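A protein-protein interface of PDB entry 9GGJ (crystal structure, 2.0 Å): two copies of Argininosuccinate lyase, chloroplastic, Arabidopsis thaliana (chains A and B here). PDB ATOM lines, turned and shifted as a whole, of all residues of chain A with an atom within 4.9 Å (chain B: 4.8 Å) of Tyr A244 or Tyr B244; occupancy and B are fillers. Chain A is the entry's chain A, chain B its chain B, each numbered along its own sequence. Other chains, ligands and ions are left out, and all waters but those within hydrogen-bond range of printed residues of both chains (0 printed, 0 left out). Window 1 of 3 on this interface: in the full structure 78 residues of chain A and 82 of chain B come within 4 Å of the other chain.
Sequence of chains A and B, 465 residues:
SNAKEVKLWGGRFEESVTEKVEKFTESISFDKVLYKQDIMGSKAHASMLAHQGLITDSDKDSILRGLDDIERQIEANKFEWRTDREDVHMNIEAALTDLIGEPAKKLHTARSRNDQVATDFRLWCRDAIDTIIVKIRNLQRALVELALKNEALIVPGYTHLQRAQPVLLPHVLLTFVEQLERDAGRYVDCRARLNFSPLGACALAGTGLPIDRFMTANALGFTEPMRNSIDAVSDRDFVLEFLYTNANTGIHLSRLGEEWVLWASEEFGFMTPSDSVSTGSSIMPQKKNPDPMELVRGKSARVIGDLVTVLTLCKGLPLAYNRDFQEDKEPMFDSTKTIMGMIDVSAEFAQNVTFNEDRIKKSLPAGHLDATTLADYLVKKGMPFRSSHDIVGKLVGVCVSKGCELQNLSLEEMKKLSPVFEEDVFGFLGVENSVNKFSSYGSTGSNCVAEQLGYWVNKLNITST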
ATOM      1  N   ARG A 186     -24.242 -16.562  36.171  1.00  0.00           N
ATOM      2  CA  ARG A 186     -24.304 -16.489  34.716  1.00  0.00           C
ATOM      3  C   ARG A 186     -23.528 -17.624  34.049  1.00  0.00           C
ATOM      4  O   ARG A 186     -24.003 -18.155  33.046  1.00  0.00           O
ATOM      5  CB  ARG A 186     -23.790 -15.148  34.173  1.00  0.00           C
ATOM      6  CG  ARG A 186     -24.753 -13.992  34.400  1.00  0.00           C
ATOM      7  CD  ARG A 186     -24.336 -12.667  33.757  1.00  0.00           C
ATOM      8  NE  ARG A 186     -23.545 -11.845  34.677  1.00  0.00           N
ATOM      9  CZ  ARG A 186     -23.997 -11.141  35.724  1.00  0.00           C
ATOM     10  NH1 ARG A 186     -25.298 -10.992  35.942  1.00  0.00           N
ATOM     11  NH2 ARG A 186     -23.145 -10.600  36.581  1.00  0.00           N
ATOM     12  N   ASP A 237     -24.558 -18.847  19.596  1.00  0.00           N
ATOM     13  CA  ASP A 237     -25.045 -18.100  20.740  1.00  0.00           C
ATOM     14  C   ASP A 237     -24.157 -18.410  21.933  1.00  0.00           C
ATOM     15  O   ASP A 237     -23.962 -17.554  22.789  1.00  0.00           O
ATOM     16  CB  ASP A 237     -26.461 -18.485  21.130  1.00  0.00           C
ATOM     17  CG  ASP A 237     -27.535 -18.050  20.142  1.00  0.00           C
ATOM     18  OD1 ASP A 237     -27.213 -17.261  19.159  1.00  0.00           O
ATOM     19  OD2 ASP A 237     -28.699 -18.466  20.388  1.00  0.00           O
ATOM     20  N   LEU A 240     -21.432 -16.003  22.017  1.00  0.00           N
ATOM     21  CA  LEU A 240     -21.930 -14.688  22.418  1.00  0.00           C
ATOM     22  C   LEU A 240     -22.204 -14.612  23.928  1.00  0.00           C
ATOM     23  O   LEU A 240     -21.829 -13.615  24.576  1.00  0.00           O
ATOM     24  CB  LEU A 240     -23.181 -14.299  21.616  1.00  0.00           C
ATOM     25  CG  LEU A 240     -23.006 -14.122  20.107  1.00  0.00           C
ATOM     26  CD1 LEU A 240     -24.350 -13.992  19.460  1.00  0.00           C
ATOM     27  CD2 LEU A 240     -22.174 -12.916  19.746  1.00  0.00           C
ATOM     28  N   GLU A 241     -22.869 -15.610  24.502  1.00  0.00           N
ATOM     29  CA  GLU A 241     -23.255 -15.555  25.910  1.00  0.00           C
ATOM     30  C   GLU A 241     -22.040 -15.676  26.860  1.00  0.00           C
ATOM     31  O   GLU A 241     -21.988 -15.103  27.966  1.00  0.00           O
ATOM     32  CB  GLU A 241     -24.269 -16.680  26.138  1.00  0.00           C
ATOM     33  CG  GLU A 241     -24.837 -16.669  27.557  1.00  0.00           C
ATOM     34  CD  GLU A 241     -26.030 -17.580  27.789  1.00  0.00           C
ATOM     35  OE1 GLU A 241     -26.551 -18.230  26.841  1.00  0.00           O
ATOM     36  OE2 GLU A 241     -26.429 -17.619  28.984  1.00  0.00           O
ATOM     37  N   PHE A 242     -21.049 -16.462  26.430  1.00  0.00           N
ATOM     38  CA  PHE A 242     -19.816 -16.633  27.201  1.00  0.00           C
ATOM     39  C   PHE A 242     -18.970 -15.372  27.084  1.00  0.00           C
ATOM     40  O   PHE A 242     -18.312 -14.975  28.041  1.00  0.00           O
ATOM     41  CB  PHE A 242     -19.162 -17.905  26.659  1.00  0.00           C
ATOM     42  CG  PHE A 242     -17.913 -18.401  27.362  1.00  0.00           C
ATOM     43  CD1 PHE A 242     -17.552 -17.936  28.642  1.00  0.00           C
ATOM     44  CD2 PHE A 242     -17.094 -19.352  26.740  1.00  0.00           C
ATOM     45  CE1 PHE A 242     -16.402 -18.403  29.264  1.00  0.00           C
ATOM     46  CE2 PHE A 242     -15.964 -19.839  27.380  1.00  0.00           C
ATOM     47  CZ  PHE A 242     -15.617 -19.360  28.640  1.00  0.00           C
ATOM     48  N   LEU A 243     -18.971 -14.719  25.921  1.00  0.00           N
ATOM     49  CA  LEU A 243     -18.247 -13.466  25.780  1.00  0.00           C
ATOM     50  C   LEU A 243     -18.842 -12.387  26.678  1.00  0.00           C
ATOM     51  O   LEU A 243     -18.087 -11.636  27.308  1.00  0.00           O
ATOM     52  CB  LEU A 243     -18.247 -13.029  24.322  1.00  0.00           C
ATOM     53  CG  LEU A 243     -17.399 -13.860  23.352  1.00  0.00           C
ATOM     54  CD1 LEU A 243     -17.815 -13.533  21.933  1.00  0.00           C
ATOM     55  CD2 LEU A 243     -15.931 -13.679  23.513  1.00  0.00           C
ATOM     56  N   TYR A 244     -20.179 -12.307  26.700  1.00  0.00           N
ATOM     57  CA  TYR A 244     -20.920 -11.349  27.512  1.00  0.00           C
ATOM     58  C   TYR A 244     -20.609 -11.620  28.990  1.00  0.00           C
ATOM     59  O   TYR A 244     -20.257 -10.691  29.719  1.00  0.00           O
ATOM     60  CB  TYR A 244     -22.439 -11.227  27.249  1.00  0.00           C
ATOM     61  CG  TYR A 244     -23.138 -10.682  28.479  1.00  0.00           C
ATOM     62  CD1 TYR A 244     -23.049  -9.345  28.836  1.00  0.00           C
ATOM     63  CD2 TYR A 244     -23.778 -11.534  29.347  1.00  0.00           C
ATOM     64  CE1 TYR A 244     -23.581  -8.873  30.028  1.00  0.00           C
ATOM     65  CE2 TYR A 244     -24.305 -11.086  30.545  1.00  0.00           C
ATOM     66  CZ  TYR A 244     -24.172  -9.763  30.899  1.00  0.00           C
ATOM     67  OH  TYR A 244     -24.691  -9.393  32.102  1.00  0.00           O
ATOM     68  N   THR A 245     -20.697 -12.877  29.435  1.00  0.00           N
ATOM     69  CA  THR A 245     -20.465 -13.195  30.830  1.00  0.00           C
ATOM     70  C   THR A 245     -19.040 -12.842  31.257  1.00  0.00           C
ATOM     71  O   THR A 245     -18.859 -12.305  32.352  1.00  0.00           O
ATOM     72  CB  THR A 245     -20.731 -14.662  31.123  1.00  0.00           C
ATOM     73  OG1 THR A 245     -22.044 -14.809  30.619  1.00  0.00           O
ATOM     74  CG2 THR A 245     -20.644 -14.942  32.616  1.00  0.00           C
ATOM     75  N   ASN A 246     -18.048 -13.113  30.392  1.00  0.00           N
ATOM     76  CA  ASN A 246     -16.674 -12.664  30.633  1.00  0.00           C
ATOM     77  C   ASN A 246     -16.644 -11.142  30.753  1.00  0.00           C
ATOM     78  O   ASN A 246     -15.962 -10.616  31.620  1.00  0.00           O
ATOM     79  CB  ASN A 246     -15.669 -13.120  29.566  1.00  0.00           C
ATOM     80  CG  ASN A 246     -15.443 -14.610  29.589  1.00  0.00           C
ATOM     81  OD1 ASN A 246     -15.812 -15.296  30.555  1.00  0.00           O
ATOM     82  ND2 ASN A 246     -14.857 -15.138  28.526  1.00  0.00           N
ATOM     83  N   ALA A 247     -17.412 -10.444  29.910  1.00  0.00           N
ATOM     84  CA  ALA A 247     -17.351  -8.984  29.865  1.00  0.00           C
ATOM     85  C   ALA A 247     -17.902  -8.365  31.139  1.00  0.00           C
ATOM     86  O   ALA A 247     -17.366  -7.354  31.579  1.00  0.00           O
ATOM     87  CB  ALA A 247     -18.100  -8.444  28.678  1.00  0.00           C
ATOM     88  N   ASN A 248     -18.985  -8.943  31.675  1.00  0.00           N
ATOM     89  CA  ASN A 248     -19.588  -8.434  32.896  1.00  0.00           C
ATOM     90  C   ASN A 248     -18.662  -8.751  34.091  1.00  0.00           C
ATOM     91  O   ASN A 248     -18.541  -7.961  35.016  1.00  0.00           O
ATOM     92  CB  ASN A 248     -20.971  -9.029  33.100  1.00  0.00           C
ATOM     93  CG  ASN A 248     -21.879  -8.230  34.004  1.00  0.00           C
ATOM     94  OD1 ASN A 248     -21.427  -7.606  34.978  1.00  0.00           O
ATOM     95  ND2 ASN A 248     -23.157  -8.180  33.647  1.00  0.00           N
ATOM     96  N   LEU A 307     -16.410  -9.303  22.602  1.00  0.00           N
ATOM     97  CA  LEU A 307     -17.844  -9.478  22.526  1.00  0.00           C
ATOM     98  C   LEU A 307     -18.433  -8.727  21.327  1.00  0.00           C
ATOM     99  O   LEU A 307     -19.173  -9.293  20.525  1.00  0.00           O
ATOM    100  CB  LEU A 307     -18.474  -8.965  23.819  1.00  0.00           C
ATOM    101  CG  LEU A 307     -19.999  -8.816  23.792  1.00  0.00           C
ATOM    102  CD1 LEU A 307     -20.675 -10.131  23.563  1.00  0.00           C
ATOM    103  CD2 LEU A 307     -20.523  -8.172  25.078  1.00  0.00           C
ATOM    104  N   LEU A 311     -20.608 -10.203  18.091  1.00  0.00           N
ATOM    105  CA  LEU A 311     -21.947  -9.683  17.870  1.00  0.00           C
ATOM    106  C   LEU A 311     -22.073  -9.248  16.403  1.00  0.00           C
ATOM    107  O   LEU A 311     -23.005  -9.679  15.703  1.00  0.00           O
ATOM    108  CB  LEU A 311     -22.378  -8.554  18.807  1.00  0.00           C
ATOM    109  CG  LEU A 311     -22.696  -8.973  20.253  1.00  0.00           C
ATOM    110  CD1 LEU A 311     -22.854  -7.823  21.236  1.00  0.00           C
ATOM    111  CD2 LEU A 311     -23.935  -9.800  20.300  1.00  0.00           C
ATOM    112  N   ARG B 186     -32.818 -17.120  28.197  1.00  0.00           N
ATOM    113  CA  ARG B 186     -31.961 -16.112  28.767  1.00  0.00           C
ATOM    114  C   ARG B 186     -32.779 -15.053  29.486  1.00  0.00           C
ATOM    115  O   ARG B 186     -32.283 -14.513  30.465  1.00  0.00           O
ATOM    116  CB  ARG B 186     -31.035 -15.504  27.719  1.00  0.00           C
ATOM    117  CG  ARG B 186     -29.897 -16.403  27.278  1.00  0.00           C
ATOM    118  CD  ARG B 186     -29.039 -15.596  26.318  1.00  0.00           C
ATOM    119  NE  ARG B 186     -29.485 -15.673  24.930  1.00  0.00           N
ATOM    120  CZ  ARG B 186     -29.198 -16.679  24.120  1.00  0.00           C
ATOM    121  NH1 ARG B 186     -28.291 -17.565  24.496  1.00  0.00           N
ATOM    122  NH2 ARG B 186     -29.800 -16.804  22.944  1.00  0.00           N
ATOM    123  N   ASP B 237     -25.856  -4.844  36.955  1.00  0.00           N
ATOM    124  CA  ASP B 237     -25.703  -6.110  36.195  1.00  0.00           C
ATOM    125  C   ASP B 237     -27.016  -6.488  35.518  1.00  0.00           C
ATOM    126  O   ASP B 237     -26.977  -6.998  34.409  1.00  0.00           O
ATOM    127  CB  ASP B 237     -25.358  -7.276  37.118  1.00  0.00           C
ATOM    128  CG  ASP B 237     -23.908  -7.319  37.566  1.00  0.00           C
ATOM    129  OD1 ASP B 237     -23.160  -6.380  37.240  1.00  0.00           O
ATOM    130  OD2 ASP B 237     -23.548  -8.295  38.234  1.00  0.00           O
ATOM    131  N   LEU B 240     -27.183  -4.705  32.210  1.00  0.00           N
ATOM    132  CA  LEU B 240     -26.245  -5.301  31.274  1.00  0.00           C
ATOM    133  C   LEU B 240     -26.770  -6.620  30.705  1.00  0.00           C
ATOM    134  O   LEU B 240     -26.610  -6.872  29.510  1.00  0.00           O
ATOM    135  CB  LEU B 240     -24.891  -5.516  31.970  1.00  0.00           C
ATOM    136  CG  LEU B 240     -24.098  -4.245  32.271  1.00  0.00           C
ATOM    137  CD1 LEU B 240     -22.747  -4.531  32.913  1.00  0.00           C
ATOM    138  CD2 LEU B 240     -23.859  -3.400  31.028  1.00  0.00           C
ATOM    139  N   GLU B 241     -27.331  -7.467  31.572  1.00  0.00           N
ATOM    140  CA  GLU B 241     -27.773  -8.801  31.191  1.00  0.00           C
ATOM    141  C   GLU B 241     -29.007  -8.691  30.294  1.00  0.00           C
ATOM    142  O   GLU B 241     -29.152  -9.455  29.325  1.00  0.00           O
ATOM    143  CB  GLU B 241     -28.065  -9.659  32.433  1.00  0.00           C
ATOM    144  CG  GLU B 241     -28.407 -11.116  32.110  1.00  0.00           C
ATOM    145  CD  GLU B 241     -28.377 -12.142  33.266  1.00  0.00           C
ATOM    146  OE1 GLU B 241     -27.988 -11.748  34.406  1.00  0.00           O
ATOM    147  OE2 GLU B 241     -28.757 -13.347  33.011  1.00  0.00           O
ATOM    148  N   PHE B 242     -29.888  -7.735  30.609  1.00  0.00           N
ATOM    149  CA  PHE B 242     -31.064  -7.489  29.790  1.00  0.00           C
ATOM    150  C   PHE B 242     -30.647  -6.993  28.399  1.00  0.00           C
ATOM    151  O   PHE B 242     -31.071  -7.558  27.392  1.00  0.00           O
ATOM    152  CB  PHE B 242     -31.996  -6.586  30.602  1.00  0.00           C
ATOM    153  CG  PHE B 242     -33.408  -6.333  30.089  1.00  0.00           C
ATOM    154  CD1 PHE B 242     -33.918  -7.002  28.985  1.00  0.00           C
ATOM    155  CD2 PHE B 242     -34.256  -5.426  30.751  1.00  0.00           C
ATOM    156  CE1 PHE B 242     -35.200  -6.718  28.510  1.00  0.00           C
ATOM    157  CE2 PHE B 242     -35.547  -5.177  30.298  1.00  0.00           C
ATOM    158  CZ  PHE B 242     -36.010  -5.826  29.180  1.00  0.00           C
ATOM    159  N   LEU B 243     -29.810  -5.953  28.347  1.00  0.00           N
ATOM    160  CA  LEU B 243     -29.287  -5.420  27.090  1.00  0.00           C
ATOM    161  C   LEU B 243     -28.656  -6.530  26.233  1.00  0.00           C
ATOM    162  O   LEU B 243     -28.795  -6.557  25.003  1.00  0.00           O
ATOM    163  CB  LEU B 243     -28.297  -4.286  27.387  1.00  0.00           C
ATOM    164  CG  LEU B 243     -28.927  -3.011  27.963  1.00  0.00           C
ATOM    165  CD1 LEU B 243     -27.956  -2.179  28.775  1.00  0.00           C
ATOM    166  CD2 LEU B 243     -29.529  -2.142  26.910  1.00  0.00           C
ATOM    167  N   TYR B 244     -27.909  -7.426  26.897  1.00  0.00           N
ATOM    168  CA  TYR B 244     -27.198  -8.465  26.173  1.00  0.00           C
ATOM    169  C   TYR B 244     -28.267  -9.384  25.600  1.00  0.00           C
ATOM    170  O   TYR B 244     -28.276  -9.684  24.416  1.00  0.00           O
ATOM    171  CB  TYR B 244     -26.174  -9.232  27.021  1.00  0.00           C
ATOM    172  CG  TYR B 244     -25.944 -10.559  26.334  1.00  0.00           C
ATOM    173  CD1 TYR B 244     -25.327 -10.609  25.090  1.00  0.00           C
ATOM    174  CD2 TYR B 244     -26.462 -11.719  26.878  1.00  0.00           C
ATOM    175  CE1 TYR B 244     -25.210 -11.812  24.408  1.00  0.00           C
ATOM    176  CE2 TYR B 244     -26.345 -12.918  26.220  1.00  0.00           C
ATOM    177  CZ  TYR B 244     -25.725 -12.961  24.981  1.00  0.00           C
ATOM    178  OH  TYR B 244     -25.660 -14.176  24.358  1.00  0.00           O
ATOM    179  N   THR B 245     -29.222  -9.765  26.443  1.00  0.00           N
ATOM    180  CA  THR B 245     -30.259 -10.673  25.984  1.00  0.00           C
ATOM    181  C   THR B 245     -31.035 -10.060  24.796  1.00  0.00           C
ATOM    182  O   THR B 245     -31.285 -10.767  23.815  1.00  0.00           O
ATOM    183  CB  THR B 245     -31.181 -11.105  27.132  1.00  0.00           C
ATOM    184  OG1 THR B 245     -30.317 -11.566  28.165  1.00  0.00           O
ATOM    185  CG2 THR B 245     -32.085 -12.211  26.656  1.00  0.00           C
ATOM    186  N   ASN B 246     -31.399  -8.774  24.878  1.00  0.00           N
ATOM    187  CA  ASN B 246     -31.999  -8.103  23.733  1.00  0.00           C
ATOM    188  C   ASN B 246     -31.124  -8.241  22.469  1.00  0.00           C
ATOM    189  O   ASN B 246     -31.614  -8.530  21.360  1.00  0.00           O
ATOM    190  CB  ASN B 246     -32.334  -6.644  24.042  1.00  0.00           C
ATOM    191  CG  ASN B 246     -33.478  -6.520  25.022  1.00  0.00           C
ATOM    192  OD1 ASN B 246     -34.134  -7.521  25.341  1.00  0.00           O
ATOM    193  ND2 ASN B 246     -33.730  -5.320  25.530  1.00  0.00           N
ATOM    194  N   ALA B 247     -29.813  -8.028  22.622  1.00  0.00           N
ATOM    195  CA  ALA B 247     -28.917  -7.962  21.469  1.00  0.00           C
ATOM    196  C   ALA B 247     -28.771  -9.322  20.794  1.00  0.00           C
ATOM    197  O   ALA B 247     -28.755  -9.407  19.568  1.00  0.00           O
ATOM    198  CB  ALA B 247     -27.577  -7.401  21.896  1.00  0.00           C
ATOM    199  N   ASN B 248     -28.722 -10.392  21.588  1.00  0.00           N
ATOM    200  CA  ASN B 248     -28.652 -11.709  21.003  1.00  0.00           C
ATOM    201  C   ASN B 248     -29.951 -12.011  20.264  1.00  0.00           C
ATOM    202  O   ASN B 248     -29.899 -12.605  19.180  1.00  0.00           O
ATOM    203  CB  ASN B 248     -28.316 -12.791  22.024  1.00  0.00           C
ATOM    204  CG  ASN B 248     -27.686 -13.989  21.354  1.00  0.00           C
ATOM    205  OD1 ASN B 248     -28.117 -14.446  20.276  1.00  0.00           O
ATOM    206  ND2 ASN B 248     -26.688 -14.560  21.983  1.00  0.00           N
ATOM    207  N   LEU B 307     -26.094  -1.846  24.348  1.00  0.00           N
ATOM    208  CA  LEU B 307     -25.378  -2.733  25.249  1.00  0.00           C
ATOM    209  C   LEU B 307     -23.980  -2.160  25.528  1.00  0.00           C
ATOM    210  O   LEU B 307     -23.557  -2.083  26.675  1.00  0.00           O
ATOM    211  CB  LEU B 307     -25.304  -4.109  24.582  1.00  0.00           C
ATOM    212  CG  LEU B 307     -24.310  -5.091  25.208  1.00  0.00           C
ATOM    213  CD1 LEU B 307     -24.726  -5.403  26.654  1.00  0.00           C
ATOM    214  CD2 LEU B 307     -24.242  -6.327  24.308  1.00  0.00           C
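Among the printed residues, pairs that only touch across the chains: Leu A240 with Asn B248 (3.5 Å), Leu A240 with Tyr B244 (3.5 Å), Tyr A244 with Tyr B244 (3.5 Å), Asn A248 with Leu B240 (3.6 Å), Tyr A244 with Leu B240 (3.7 Å) and Leu A311 with Leu B307 (3.7 Å).
Asp A237 touches Asn B248, and with the chains exchanged Asn A248 touches Asp B237.
Leu A240 touches Tyr B244, and with the chains exchanged Tyr A244 touches Leu B240.
Glu A241 touches Tyr B244, and with the chains exchanged Tyr A244 touches Glu B241.
Tyr B244 touches its own counterpart, Tyr A244.
Positions printed for both chains: 186, 237, 240, 241, 242, 243, 244, 245, 246, 247, 248 and 307.
Of the 14 pairs that touch across the chains among the printed residues, 13 have their exchanged pair printed and touching as well.
NH1 of Arg B186 lies within salt-bridge range of OE1 of Glu A241, at 3.0 Å.
OD2 of Asp A237 is in salt-bridge range of NH2 of Arg B186 (3.2 Å).
The guanidinium group (NH2) of Arg A186 lies within salt-bridge range of the side-chain carboxylate (OD2) of Asp B237.
NH1 of Arg A186 lies within salt-bridge range of OE1 of Glu B241 (3.2 Å).
OH of Tyr A244 sits close to N of Glu B241, 3.3 Å away.
OD1 of Asp A237 sits close to OD1 of Asn B248, at 3.2 Å.
OD1 of Asp B237 sits close to OD1 of Asn A248, 3.1 Å away.
The side-chain hydroxyl of Tyr B244 sits at hydrogen-bond distance from the backbone NH of Glu A241, at 3.1 Å.
Of chain B, only Leu B240, Glu B241 and Tyr B244 come within 4 Å of Tyr A244.
Of the printed residues of chain A, Asp B237 touches Arg A186 (2.9 Å) and Asn A248 (3.1 Å).
Printed residues of chain A within 4 Å of Leu B240: Tyr A244 and Asn A248.
Tyr B244 touches three residues of chain A.
Of the printed residues of chain A, Asn B248 touches Asp A237 and Leu A240.
Of the printed residues of chain A, Leu B307 touches Leu A311.
The nearest residue of chain A that does not touch Tyr B244 is Asp A237 (4.1 Å).
Of the 12 printed residues of chain B, 7 touch a printed residue of chain A.
Hydrophobic or aromatic side chains of chain B that line the printed part of chain A: Leu B240, Tyr B244 and Leu B307.
Printed residues of chain A that touch a printed residue of chain B: Arg A186, Asp A237, Leu A240, Glu A241, Tyr A244, Asn A248 and Leu A311.
Among the printed residues, 14 pairs touch across the chains.
Among the printed residues, Asp or Glu carboxylates within 4 Å of a Lys or Arg side-chain nitrogen of the other chain: Arg A186 with Asp B237 (2.9 Å), Arg A186 with Glu B241 (3.2 Å), Asp A237 with Arg B186 (3.2 Å) and Glu A241 with Arg B186 (3.0 Å).
O of Glu A241 lies within hydrogen-bond range of OG1 of Thr A245, at 2.7 Å.
The side-chain hydroxyl (OG1) of Thr B245 sits at hydrogen-bond distance from the backbone carbonyl oxygen (O) of Glu B241 (2.7 Å).
The side-chain amide nitrogen (ND2) of Asn B248 sits at hydrogen-bond distance from the side-chain hydroxyl (OH) of Tyr B244 (2.6 Å).
The side-chain amide nitrogen of Asn A248 is in hydrogen-bond range of the side-chain hydroxyl of Tyr A244.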
